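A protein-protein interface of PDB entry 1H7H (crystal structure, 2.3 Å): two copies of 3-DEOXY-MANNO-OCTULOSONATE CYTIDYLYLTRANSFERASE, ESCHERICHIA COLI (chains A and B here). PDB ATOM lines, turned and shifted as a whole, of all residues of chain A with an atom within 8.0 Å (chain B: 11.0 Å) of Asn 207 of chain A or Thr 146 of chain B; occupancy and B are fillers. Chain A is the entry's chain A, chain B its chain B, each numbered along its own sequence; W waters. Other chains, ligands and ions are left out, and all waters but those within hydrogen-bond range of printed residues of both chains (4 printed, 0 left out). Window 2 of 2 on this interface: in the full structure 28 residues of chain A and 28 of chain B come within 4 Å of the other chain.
O of Asn 207 of chain A lies within hydrogen-bond range of N of Thr 146 of chain B (3.3 Å).
The backbone carbonyl oxygen of Val 143 of chain B is in hydrogen-bond range of the backbone NH of Leu 151 of chain B (2.7 Å). The backbone NH of Gln 148 of chain B lies within hydrogen-bond range of the side-chain amide oxygen of Asn 145 of chain B (3.1 Å). The backbone NH of Val 143 of chain B is in hydrogen-bond range of the backbone carbonyl oxygen of Tyr 152 of chain B. OD1 of Asn 145 of chain B is in hydrogen-bond range of N of Asp 149 of chain B (2.9 Å). The side-chain amide oxygen (OD1) of Asn 145 of chain B lies within hydrogen-bond range of the backbone NH (N) of Arg 147 of chain B.
Among the printed residues, merely in contact across the chains: Met 193 of chain A with Pro 159 of chain B (3.9 Å), Pro 194 of chain A with Val 143 of chain B (3.8 Å), Met 206 of chain A with Asn 145 of chain B (3.8 Å) and Asn 207 of chain A with Asn 145 of chain B (3.3 Å).
Of the printed residues of chain B, Asn 207 of chain A touches Asn 145 (3.3 Å) and Thr 146 (3.1 Å). Thr 146 of chain B touches one residue of chain A. No residue of chain B comes within 4 Å of Pro 190 of chain A. No residue of chain B comes within 4 Å of Ser 192 of chain A. No residue of chain B comes within 4 Å of Ala 208 of chain A. No residue of chain B comes within 4 Å of Gly 209 of chain A. Of the printed residues of chain B, Met 193 of chain A touches Pro 159. Of the printed residues of chain A, Pro 159 of chain B touches Met 193 (3.9 Å). Leu 189 of chain A touches none of the printed residues of chain B. Arg 213 of chain B touches none of the printed residues of chain A.
Of the 18 printed residues of chain A, 4 touch a printed residue of chain B. Among the printed residues, 5 pairs touch across the chains. Among the printed residues, no Asp or Glu carboxylate lies within 4 Å of a Lys or Arg side-chain nitrogen of the other chain.
1 position is printed for both chains. Of the 5 pairs that touch across the chains among the printed residues, none has its exchanged pair printed and touching as well.
Water W2 lies within hydrogen-bond range of the backbone carbonyl oxygen (O) of Met 206 of chain A (2.7 Å) and the side-chain amide nitrogen (ND2) of Asn 145 of chain B (3.1 Å). Water W1 bridges the side-chain amide oxygen of Asn 207 of chain A (2.7 Å) and the backbone carbonyl oxygen of Val 144 of chain B (2.7 Å). Water W3 lies within hydrogen-bond range of OG1 of Thr 146 of chain B, O of Asn 207 of chain A and N of Arg 147 of chain B. Water W4 bridges the side-chain amide oxygen (OD1) of Asn 207 of chain A (2.9 Å) and the backbone NH (N) of Thr 146 of chain B (3.5 Å).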
ATOM      1  N   LEU A 189     -38.018  17.098 -11.247  1.00  0.00           N
ATOM      2  CA  LEU A 189     -36.914  18.028 -11.022  1.00  0.00           C
ATOM      3  C   LEU A 189     -36.815  19.085 -12.120  1.00  0.00           C
ATOM      4  O   LEU A 189     -36.869  18.775 -13.313  1.00  0.00           O
ATOM      5  CB  LEU A 189     -35.587  17.276 -10.944  1.00  0.00           C
ATOM      6  CG  LEU A 189     -35.424  16.252  -9.825  1.00  0.00           C
ATOM      7  CD1 LEU A 189     -34.024  15.671  -9.882  1.00  0.00           C
ATOM      8  CD2 LEU A 189     -35.680  16.918  -8.482  1.00  0.00           C
ATOM      9  N   PRO A 190     -36.705  20.360 -11.728  1.00  0.00           N
ATOM     10  CA  PRO A 190     -36.600  21.406 -12.748  1.00  0.00           C
ATOM     11  C   PRO A 190     -35.158  21.508 -13.244  1.00  0.00           C
ATOM     12  O   PRO A 190     -34.232  21.029 -12.584  1.00  0.00           O
ATOM     13  CB  PRO A 190     -37.021  22.659 -11.980  1.00  0.00           C
ATOM     14  CG  PRO A 190     -36.493  22.393 -10.594  1.00  0.00           C
ATOM     15  CD  PRO A 190     -36.827  20.935 -10.372  1.00  0.00           C
ATOM     16  N   GLU A 191     -34.974  22.070 -14.435  1.00  0.00           N
ATOM     17  CA  GLU A 191     -33.632  22.255 -14.978  1.00  0.00           C
ATOM     18  C   GLU A 191     -32.969  23.379 -14.182  1.00  0.00           C
ATOM     19  O   GLU A 191     -33.637  24.323 -13.762  1.00  0.00           O
ATOM     20  CB  GLU A 191     -33.698  22.645 -16.454  1.00  0.00           C
ATOM     21  CG  GLU A 191     -34.165  21.534 -17.376  1.00  0.00           C
ATOM     22  CD  GLU A 191     -34.164  21.951 -18.835  1.00  0.00           C
ATOM     23  OE1 GLU A 191     -33.160  22.538 -19.296  1.00  0.00           O
ATOM     24  OE2 GLU A 191     -35.172  21.693 -19.524  1.00  0.00           O
ATOM     25  N   SER A 192     -31.671  23.256 -13.935  1.00  0.00           N
ATOM     26  CA  SER A 192     -30.954  24.277 -13.188  1.00  0.00           C
ATOM     27  C   SER A 192     -30.164  25.173 -14.128  1.00  0.00           C
ATOM     28  O   SER A 192     -29.851  24.790 -15.261  1.00  0.00           O
ATOM     29  CB  SER A 192     -30.013  23.638 -12.168  1.00  0.00           C
ATOM     30  OG  SER A 192     -28.985  22.900 -12.806  1.00  0.00           O
ATOM     31  N   MET A 193     -29.843  26.369 -13.644  1.00  0.00           N
ATOM     32  CA  MET A 193     -29.075  27.336 -14.412  1.00  0.00           C
ATOM     33  C   MET A 193     -27.679  26.765 -14.741  1.00  0.00           C
ATOM     34  O   MET A 193     -27.238  26.846 -15.888  1.00  0.00           O
ATOM     35  CB  MET A 193     -29.005  28.668 -13.651  1.00  0.00           C
ATOM     36  CG  MET A 193     -28.187  29.766 -14.320  1.00  0.00           C
ATOM     37  SD  MET A 193     -26.421  29.484 -14.150  1.00  0.00           S
ATOM     38  CE  MET A 193     -26.240  29.817 -12.398  1.00  0.00           C
ATOM     39  N   PRO A 194     -26.971  26.180 -13.748  1.00  0.00           N
ATOM     40  CA  PRO A 194     -25.643  25.622 -14.045  1.00  0.00           C
ATOM     41  C   PRO A 194     -25.733  24.509 -15.097  1.00  0.00           C
ATOM     42  O   PRO A 194     -24.890  24.421 -15.996  1.00  0.00           O
ATOM     43  CB  PRO A 194     -25.189  25.077 -12.688  1.00  0.00           C
ATOM     44  CG  PRO A 194     -25.824  26.034 -11.723  1.00  0.00           C
ATOM     45  CD  PRO A 194     -27.228  26.152 -12.294  1.00  0.00           C
ATOM     46  N   GLU A 195     -26.780  23.689 -15.001  1.00  0.00           N
ATOM     47  CA  GLU A 195     -26.993  22.599 -15.951  1.00  0.00           C
ATOM     48  C   GLU A 195     -27.117  23.142 -17.371  1.00  0.00           C
ATOM     49  O   GLU A 195     -26.467  22.647 -18.290  1.00  0.00           O
ATOM     50  CB  GLU A 195     -28.272  21.828 -15.619  1.00  0.00           C
ATOM     51  CG  GLU A 195     -28.574  20.742 -16.648  1.00  0.00           C
ATOM     52  CD  GLU A 195     -30.020  20.282 -16.668  1.00  0.00           C
ATOM     53  OE1 GLU A 195     -30.753  20.501 -15.674  1.00  0.00           O
ATOM     54  OE2 GLU A 195     -30.414  19.684 -17.693  1.00  0.00           O
ATOM     55  N   GLU A 201     -26.134  17.327 -17.739  1.00  0.00           N
ATOM     56  CA  GLU A 201     -27.362  16.877 -17.104  1.00  0.00           C
ATOM     57  C   GLU A 201     -27.234  16.476 -15.639  1.00  0.00           C
ATOM     58  O   GLU A 201     -28.180  16.668 -14.871  1.00  0.00           O
ATOM     59  CB  GLU A 201     -28.002  15.753 -17.911  1.00  0.00           C
ATOM     60  CG  GLU A 201     -29.425  15.431 -17.473  1.00  0.00           C
ATOM     61  CD  GLU A 201     -30.108  14.373 -18.330  1.00  0.00           C
ATOM     62  OE1 GLU A 201     -29.407  13.497 -18.895  1.00  0.00           O
ATOM     63  OE2 GLU A 201     -31.357  14.414 -18.425  1.00  0.00           O
ATOM     64  N   GLN A 202     -26.070  15.972 -15.231  1.00  0.00           N
ATOM     65  CA  GLN A 202     -25.886  15.559 -13.834  1.00  0.00           C
ATOM     66  C   GLN A 202     -26.001  16.707 -12.819  1.00  0.00           C
ATOM     67  O   GLN A 202     -26.192  16.469 -11.629  1.00  0.00           O
ATOM     68  CB  GLN A 202     -24.569  14.799 -13.632  1.00  0.00           C
ATOM     69  CG  GLN A 202     -23.300  15.601 -13.896  1.00  0.00           C
ATOM     70  CD  GLN A 202     -22.866  15.552 -15.342  1.00  0.00           C
ATOM     71  OE1 GLN A 202     -23.675  15.717 -16.248  1.00  0.00           O
ATOM     72  NE2 GLN A 202     -21.582  15.316 -15.568  1.00  0.00           N
ATOM     73  N   LEU A 203     -25.902  17.949 -13.285  1.00  0.00           N
ATOM     74  CA  LEU A 203     -26.023  19.093 -12.387  1.00  0.00           C
ATOM     75  C   LEU A 203     -27.471  19.300 -11.963  1.00  0.00           C
ATOM     76  O   LEU A 203     -27.747  20.057 -11.026  1.00  0.00           O
ATOM     77  CB  LEU A 203     -25.460  20.364 -13.028  1.00  0.00           C
ATOM     78  CG  LEU A 203     -23.949  20.320 -13.275  1.00  0.00           C
ATOM     79  CD1 LEU A 203     -23.504  21.598 -13.984  1.00  0.00           C
ATOM     80  CD2 LEU A 203     -23.197  20.117 -11.955  1.00  0.00           C
ATOM     81  N   ARG A 204     -28.401  18.632 -12.648  1.00  0.00           N
ATOM     82  CA  ARG A 204     -29.817  18.738 -12.288  1.00  0.00           C
ATOM     83  C   ARG A 204     -30.021  18.068 -10.932  1.00  0.00           C
ATOM     84  O   ARG A 204     -30.814  18.530 -10.111  1.00  0.00           O
ATOM     85  CB  ARG A 204     -30.718  18.066 -13.327  1.00  0.00           C
ATOM     86  CG  ARG A 204     -32.203  18.318 -13.079  1.00  0.00           C
ATOM     87  CD  ARG A 204     -33.079  17.753 -14.175  1.00  0.00           C
ATOM     88  NE  ARG A 204     -32.668  18.200 -15.501  1.00  0.00           N
ATOM     89  CZ  ARG A 204     -33.222  17.780 -16.636  1.00  0.00           C
ATOM     90  NH1 ARG A 204     -34.222  16.908 -16.609  1.00  0.00           N
ATOM     91  NH2 ARG A 204     -32.737  18.181 -17.801  1.00  0.00           N
ATOM     92  N   LEU A 205     -29.285  16.983 -10.704  1.00  0.00           N
ATOM     93  CA  LEU A 205     -29.355  16.237  -9.454  1.00  0.00           C
ATOM     94  C   LEU A 205     -28.729  17.036  -8.326  1.00  0.00           C
ATOM     95  O   LEU A 205     -29.283  17.119  -7.224  1.00  0.00           O
ATOM     96  CB  LEU A 205     -28.625  14.902  -9.587  1.00  0.00           C
ATOM     97  CG  LEU A 205     -29.194  13.918 -10.611  1.00  0.00           C
ATOM     98  CD1 LEU A 205     -28.231  12.759 -10.805  1.00  0.00           C
ATOM     99  CD2 LEU A 205     -30.553  13.415 -10.145  1.00  0.00           C
ATOM    100  N   MET A 206     -27.566  17.622  -8.604  1.00  0.00           N
ATOM    101  CA  MET A 206     -26.864  18.413  -7.605  1.00  0.00           C
ATOM    102  C   MET A 206     -27.658  19.641  -7.178  1.00  0.00           C
ATOM    103  O   MET A 206     -27.609  20.051  -6.016  1.00  0.00           O
ATOM    104  CB  MET A 206     -25.491  18.808  -8.121  1.00  0.00           C
ATOM    105  CG  MET A 206     -24.619  17.615  -8.395  1.00  0.00           C
ATOM    106  SD  MET A 206     -22.925  18.106  -8.489  1.00  0.00           S
ATOM    107  CE  MET A 206     -22.485  18.004  -6.779  1.00  0.00           C
ATOM    108  N   ASN A 207     -28.416  20.204  -8.112  1.00  0.00           N
ATOM    109  CA  ASN A 207     -29.245  21.372  -7.825  1.00  0.00           C
ATOM    110  C   ASN A 207     -30.310  21.024  -6.791  1.00  0.00           C
ATOM    111  O   ASN A 207     -30.652  21.844  -5.930  1.00  0.00           O
ATOM    112  CB  ASN A 207     -29.935  21.859  -9.097  1.00  0.00           C
ATOM    113  CG  ASN A 207     -30.679  23.163  -8.891  1.00  0.00           C
ATOM    114  OD1 ASN A 207     -30.096  24.154  -8.461  1.00  0.00           O
ATOM    115  ND2 ASN A 207     -31.973  23.170  -9.204  1.00  0.00           N
ATOM    116  N   ALA A 208     -30.829  19.800  -6.889  1.00  0.00           N
ATOM    117  CA  ALA A 208     -31.871  19.312  -5.992  1.00  0.00           C
ATOM    118  C   ALA A 208     -31.328  18.770  -4.671  1.00  0.00           C
ATOM    119  O   ALA A 208     -32.085  18.286  -3.839  1.00  0.00           O
ATOM    120  CB  ALA A 208     -32.710  18.251  -6.696  1.00  0.00           C
ATOM    121  N   GLY A 209     -30.019  18.844  -4.481  1.00  0.00           N
ATOM    122  CA  GLY A 209     -29.434  18.361  -3.242  1.00  0.00           C
ATOM    123  C   GLY A 209     -29.247  16.856  -3.176  1.00  0.00           C
ATOM    124  O   GLY A 209     -29.069  16.291  -2.091  1.00  0.00           O
ATOM    125  N   ILE A 210     -29.308  16.195  -4.327  1.00  0.00           N
ATOM    126  CA  ILE A 210     -29.124  14.755  -4.373  1.00  0.00           C
ATOM    127  C   ILE A 210     -27.628  14.483  -4.446  1.00  0.00           C
ATOM    128  O   ILE A 210     -26.936  14.963  -5.349  1.00  0.00           O
ATOM    129  CB  ILE A 210     -29.854  14.145  -5.585  1.00  0.00           C
ATOM    130  CG1 ILE A 210     -31.361  14.370  -5.427  1.00  0.00           C
ATOM    131  CG2 ILE A 210     -29.524  12.655  -5.719  1.00  0.00           C
ATOM    132  CD1 ILE A 210     -32.173  14.036  -6.653  1.00  0.00           C
ATOM    133  N   ILE A 212     -24.076  12.645  -4.995  1.00  0.00           N
ATOM    134  CA  ILE A 212     -23.494  11.782  -6.022  1.00  0.00           C
ATOM    135  C   ILE A 212     -22.089  11.393  -5.580  1.00  0.00           C
ATOM    136  O   ILE A 212     -21.212  12.245  -5.511  1.00  0.00           O
ATOM    137  CB  ILE A 212     -23.378  12.510  -7.381  1.00  0.00           C
ATOM    138  CG1 ILE A 212     -24.754  12.950  -7.881  1.00  0.00           C
ATOM    139  CG2 ILE A 212     -22.706  11.614  -8.404  1.00  0.00           C
ATOM    140  CD1 ILE A 212     -24.710  13.724  -9.195  1.00  0.00           C
ATOM    141  N   VAL B 143     -21.050  28.829  -6.951  1.00  0.00           N
ATOM    142  CA  VAL B 143     -22.219  28.229  -7.603  1.00  0.00           C
ATOM    143  C   VAL B 143     -23.038  27.592  -6.474  1.00  0.00           C
ATOM    144  O   VAL B 143     -22.490  26.905  -5.616  1.00  0.00           O
ATOM    145  CB  VAL B 143     -21.823  27.161  -8.666  1.00  0.00           C
ATOM    146  CG1 VAL B 143     -23.065  26.468  -9.202  1.00  0.00           C
ATOM    147  CG2 VAL B 143     -21.103  27.823  -9.827  1.00  0.00           C
ATOM    148  N   VAL B 144     -24.340  27.865  -6.458  1.00  0.00           N
ATOM    149  CA  VAL B 144     -25.233  27.358  -5.412  1.00  0.00           C
ATOM    150  C   VAL B 144     -26.376  26.479  -5.939  1.00  0.00           C
ATOM    151  O   VAL B 144     -26.629  26.430  -7.149  1.00  0.00           O
ATOM    152  CB  VAL B 144     -25.872  28.541  -4.625  1.00  0.00           C
ATOM    153  CG1 VAL B 144     -24.780  29.462  -4.064  1.00  0.00           C
ATOM    154  CG2 VAL B 144     -26.823  29.339  -5.533  1.00  0.00           C
ATOM    155  N   ASN B 145     -27.062  25.790  -5.026  1.00  0.00           N
ATOM    156  CA  ASN B 145     -28.204  24.947  -5.396  1.00  0.00           C
ATOM    157  C   ASN B 145     -29.506  25.702  -5.066  1.00  0.00           C
ATOM    158  O   ASN B 145     -29.448  26.884  -4.731  1.00  0.00           O
ATOM    159  CB  ASN B 145     -28.131  23.565  -4.717  1.00  0.00           C
ATOM    160  CG  ASN B 145     -28.224  23.634  -3.203  1.00  0.00           C
ATOM    161  OD1 ASN B 145     -28.681  24.625  -2.630  1.00  0.00           O
ATOM    162  ND2 ASN B 145     -27.816  22.559  -2.545  1.00  0.00           N
ATOM    163  N   THR B 146     -30.664  25.044  -5.164  1.00  0.00           N
ATOM    164  CA  THR B 146     -31.948  25.711  -4.887  1.00  0.00           C
ATOM    165  C   THR B 146     -32.123  26.249  -3.472  1.00  0.00           C
ATOM    166  O   THR B 146     -32.840  27.229  -3.265  1.00  0.00           O
ATOM    167  CB  THR B 146     -33.190  24.848  -5.258  1.00  0.00           C
ATOM    168  OG1 THR B 146     -33.127  23.577  -4.603  1.00  0.00           O
ATOM    169  CG2 THR B 146     -33.262  24.641  -6.743  1.00  0.00           C
ATOM    170  N   ARG B 147     -31.495  25.598  -2.497  1.00  0.00           N
ATOM    171  CA  ARG B 147     -31.559  26.057  -1.109  1.00  0.00           C
ATOM    172  C   ARG B 147     -30.463  27.092  -0.849  1.00  0.00           C
ATOM    173  O   ARG B 147     -30.245  27.494   0.294  1.00  0.00           O
ATOM    174  CB  ARG B 147     -31.376  24.897  -0.137  1.00  0.00           C
ATOM    175  CG  ARG B 147     -32.598  24.064   0.092  1.00  0.00           C
ATOM    176  CD  ARG B 147     -32.297  23.054   1.179  1.00  0.00           C
ATOM    177  NE  ARG B 147     -33.430  22.171   1.439  1.00  0.00           N
ATOM    178  CZ  ARG B 147     -33.525  21.376   2.500  1.00  0.00           C
ATOM    179  NH1 ARG B 147     -32.553  21.353   3.406  1.00  0.00           N
ATOM    180  NH2 ARG B 147     -34.590  20.598   2.648  1.00  0.00           N
ATOM    181  N   GLN B 148     -29.746  27.469  -1.907  1.00  0.00           N
ATOM    182  CA  GLN B 148     -28.669  28.455  -1.823  1.00  0.00           C
ATOM    183  C   GLN B 148     -27.401  27.967  -1.131  1.00  0.00           C
ATOM    184  O   GLN B 148     -26.582  28.764  -0.664  1.00  0.00           O
ATOM    185  CB  GLN B 148     -29.181  29.749  -1.185  1.00  0.00           C
ATOM    186  CG  GLN B 148     -30.282  30.390  -2.003  1.00  0.00           C
ATOM    187  CD  GLN B 148     -30.682  31.748  -1.488  1.00  0.00           C
ATOM    188  OE1 GLN B 148     -30.870  31.944  -0.282  1.00  0.00           O
ATOM    189  NE2 GLN B 148     -30.818  32.704  -2.402  1.00  0.00           N
ATOM    190  N   ASP B 149     -27.257  26.649  -1.048  1.00  0.00           N
ATOM    191  CA  ASP B 149     -26.074  26.045  -0.458  1.00  0.00           C
ATOM    192  C   ASP B 149     -25.007  26.079  -1.539  1.00  0.00           C
ATOM    193  O   ASP B 149     -25.301  25.861  -2.721  1.00  0.00           O
ATOM    194  CB  ASP B 149     -26.349  24.590  -0.056  1.00  0.00           C
ATOM    195  CG  ASP B 149     -27.288  24.472   1.129  1.00  0.00           C
ATOM    196  OD1 ASP B 149     -27.351  25.407   1.957  1.00  0.00           O
ATOM    197  OD2 ASP B 149     -27.949  23.419   1.247  1.00  0.00           O
ATOM    198  N   ALA B 150     -23.776  26.386  -1.148  1.00  0.00           N
ATOM    199  CA  ALA B 150     -22.685  26.446  -2.110  1.00  0.00           C
ATOM    200  C   ALA B 150     -22.268  25.049  -2.555  1.00  0.00           C
ATOM    201  O   ALA B 150     -22.154  24.135  -1.738  1.00  0.00           O
ATOM    202  CB  ALA B 150     -21.491  27.174  -1.504  1.00  0.00           C
ATOM    203  N   LEU B 151     -22.110  24.881  -3.863  1.00  0.00           N
ATOM    204  CA  LEU B 151     -21.657  23.620  -4.425  1.00  0.00           C
ATOM    205  C   LEU B 151     -20.130  23.670  -4.478  1.00  0.00           C
ATOM    206  O   LEU B 151     -19.462  22.696  -4.133  1.00  0.00           O
ATOM    207  CB  LEU B 151     -22.221  23.415  -5.833  1.00  0.00           C
ATOM    208  CG  LEU B 151     -23.731  23.185  -5.942  1.00  0.00           C
ATOM    209  CD1 LEU B 151     -24.130  23.072  -7.395  1.00  0.00           C
ATOM    210  CD2 LEU B 151     -24.119  21.934  -5.191  1.00  0.00           C
ATOM    211  N   TYR B 152     -19.582  24.825  -4.853  1.00  0.00           N
ATOM    212  CA  TYR B 152     -18.134  24.982  -4.943  1.00  0.00           C
ATOM    213  C   TYR B 152     -17.753  26.455  -5.100  1.00  0.00           C
ATOM    214  O   TYR B 152     -18.577  27.274  -5.525  1.00  0.00           O
ATOM    215  CB  TYR B 152     -17.616  24.165  -6.142  1.00  0.00           C
ATOM    216  CG  TYR B 152     -16.107  24.046  -6.247  1.00  0.00           C
ATOM    217  CD1 TYR B 152     -15.357  23.504  -5.207  1.00  0.00           C
ATOM    218  CD2 TYR B 152     -15.431  24.492  -7.387  1.00  0.00           C
ATOM    219  CE1 TYR B 152     -13.971  23.409  -5.297  1.00  0.00           C
ATOM    220  CE2 TYR B 152     -14.053  24.402  -7.482  1.00  0.00           C
ATOM    221  CZ  TYR B 152     -13.328  23.862  -6.434  1.00  0.00           C
ATOM    222  OH  TYR B 152     -11.955  23.791  -6.515  1.00  0.00           O
ATOM    223  N   PRO B 159     -20.497  28.944 -13.483  1.00  0.00           N
ATOM    224  CA  PRO B 159     -20.493  27.844 -14.455  1.00  0.00           C
ATOM    225  C   PRO B 159     -19.839  28.155 -15.799  1.00  0.00           C
ATOM    226  O   PRO B 159     -19.864  29.296 -16.271  1.00  0.00           O
ATOM    227  CB  PRO B 159     -21.980  27.557 -14.634  1.00  0.00           C
ATOM    228  CG  PRO B 159     -22.585  28.921 -14.513  1.00  0.00           C
ATOM    229  CD  PRO B 159     -21.865  29.465 -13.296  1.00  0.00           C
ATOM    230  N   LEU B 170     -21.906  34.645  -9.813  1.00  0.00           N
ATOM    231  CA  LEU B 170     -21.973  35.177  -8.457  1.00  0.00           C
ATOM    232  C   LEU B 170     -20.579  35.315  -7.891  1.00  0.00           C
ATOM    233  O   LEU B 170     -19.758  34.410  -8.025  1.00  0.00           O
ATOM    234  CB  LEU B 170     -22.785  34.252  -7.542  1.00  0.00           C
ATOM    235  CG  LEU B 170     -24.275  34.126  -7.850  1.00  0.00           C
ATOM    236  CD1 LEU B 170     -24.862  32.970  -7.077  1.00  0.00           C
ATOM    237  CD2 LEU B 170     -24.996  35.427  -7.525  1.00  0.00           C
ATOM    238  N   ASN B 211     -21.620  22.253   5.516  1.00  0.00           N
ATOM    239  CA  ASN B 211     -22.441  23.062   4.630  1.00  0.00           C
ATOM    240  C   ASN B 211     -22.247  24.568   4.824  1.00  0.00           C
ATOM    241  O   ASN B 211     -22.153  25.062   5.949  1.00  0.00           O
ATOM    242  CB  ASN B 211     -23.916  22.697   4.811  1.00  0.00           C
ATOM    243  CG  ASN B 211     -24.805  23.348   3.773  1.00  0.00           C
ATOM    244  OD1 ASN B 211     -24.528  23.275   2.575  1.00  0.00           O
ATOM    245  ND2 ASN B 211     -25.871  24.001   4.226  1.00  0.00           N
ATOM    246  N   ILE B 212     -22.229  25.291   3.712  1.00  0.00           N
ATOM    247  CA  ILE B 212     -22.066  26.738   3.723  1.00  0.00           C
ATOM    248  C   ILE B 212     -23.189  27.353   2.894  1.00  0.00           C
ATOM    249  O   ILE B 212     -23.224  27.182   1.677  1.00  0.00           O
ATOM    250  CB  ILE B 212     -20.716  27.160   3.075  1.00  0.00           C
ATOM    251  CG1 ILE B 212     -19.537  26.516   3.813  1.00  0.00           C
ATOM    252  CG2 ILE B 212     -20.596  28.686   3.053  1.00  0.00           C
ATOM    253  CD1 ILE B 212     -18.197  26.846   3.218  1.00  0.00           C
ATOM    254  N   ARG B 213     -24.130  28.032   3.545  1.00  0.00           N
ATOM    255  CA  ARG B 213     -25.212  28.663   2.802  1.00  0.00           C
ATOM    256  C   ARG B 213     -24.778  30.064   2.380  1.00  0.00           C
ATOM    257  O   ARG B 213     -24.190  30.808   3.168  1.00  0.00           O
ATOM    258  CB  ARG B 213     -26.507  28.699   3.617  1.00  0.00           C
ATOM    259  CG  ARG B 213     -27.702  29.249   2.835  1.00  0.00           C
ATOM    260  CD  ARG B 213     -29.017  28.741   3.392  1.00  0.00           C
ATOM    261  NE  ARG B 213     -29.102  27.284   3.310  1.00  0.00           N
ATOM    262  CZ  ARG B 213     -29.600  26.507   4.264  1.00  0.00           C
ATOM    263  NH1 ARG B 213     -30.076  27.042   5.383  1.00  0.00           N
ATOM    264  NH2 ARG B 213     -29.576  25.190   4.125  1.00  0.00           N
ATOM    265  N   THR B 214     -25.069  30.409   1.129  1.00  0.00           N
ATOM    266  CA  THR B 214     -24.695  31.699   0.557  1.00  0.00           C
ATOM    267  C   THR B 214     -25.897  32.595   0.264  1.00  0.00           C
ATOM    268  O   THR B 214     -26.709  32.267  -0.595  1.00  0.00           O
ATOM    269  CB  THR B 214     -23.923  31.482  -0.757  1.00  0.00           C
ATOM    270  OG1 THR B 214     -22.823  30.594  -0.522  1.00  0.00           O
ATOM    271  CG2 THR B 214     -23.383  32.792  -1.282  1.00  0.00           C
ATOM    272  N   PHE B 215     -25.982  33.736   0.949  1.00  0.00           N
ATOM    273  CA  PHE B 215     -27.077  34.692   0.764  1.00  0.00           C
ATOM    274  C   PHE B 215     -26.694  35.800  -0.211  1.00  0.00           C
ATOM    275  O   PHE B 215     -25.618  36.398  -0.097  1.00  0.00           O
ATOM    276  CB  PHE B 215     -27.484  35.304   2.106  1.00  0.00           C
ATOM    277  CG  PHE B 215     -27.962  34.293   3.112  1.00  0.00           C
ATOM    278  CD1 PHE B 215     -29.295  33.887   3.131  1.00  0.00           C
ATOM    279  CD2 PHE B 215     -27.079  33.731   4.023  1.00  0.00           C
ATOM    280  CE1 PHE B 215     -29.740  32.941   4.043  1.00  0.00           C
ATOM    281  CE2 PHE B 215     -27.516  32.785   4.937  1.00  0.00           C
ATOM    282  CZ  PHE B 215     -28.850  32.386   4.947  1.00  0.00           C
ATOM    283  N   GLU B 216     -27.598  36.101  -1.142  1.00  0.00           N
ATOM    284  CA  GLU B 216     -27.355  37.118  -2.161  1.00  0.00           C
ATOM    285  C   GLU B 216     -27.733  38.537  -1.758  1.00  0.00           C
ATOM    286  O   GLU B 216     -28.823  38.778  -1.238  1.00  0.00           O
ATOM    287  CB  GLU B 216     -28.073  36.750  -3.464  1.00  0.00           C
ATOM    288  CG  GLU B 216     -27.656  37.609  -4.651  1.00  0.00           C
ATOM    289  CD  GLU B 216     -28.361  37.241  -5.952  1.00  0.00           C
ATOM    290  OE1 GLU B 216     -28.837  36.088  -6.083  1.00  0.00           O
ATOM    291  OE2 GLU B 216     -28.423  38.109  -6.851  1.00  0.00           O
HETATM  292  O   HOH W   1     -27.454  24.550  -8.925  1.00  0.00           O
HETATM  293  O   HOH W   2     -26.604  19.868  -3.562  1.00  0.00           O
HETATM  294  O   HOH W   3     -31.383  22.261  -2.920  1.00  0.00           O
HETATM  295  O   HOH W   4     -30.717  26.957  -8.051  1.00  0.00           O
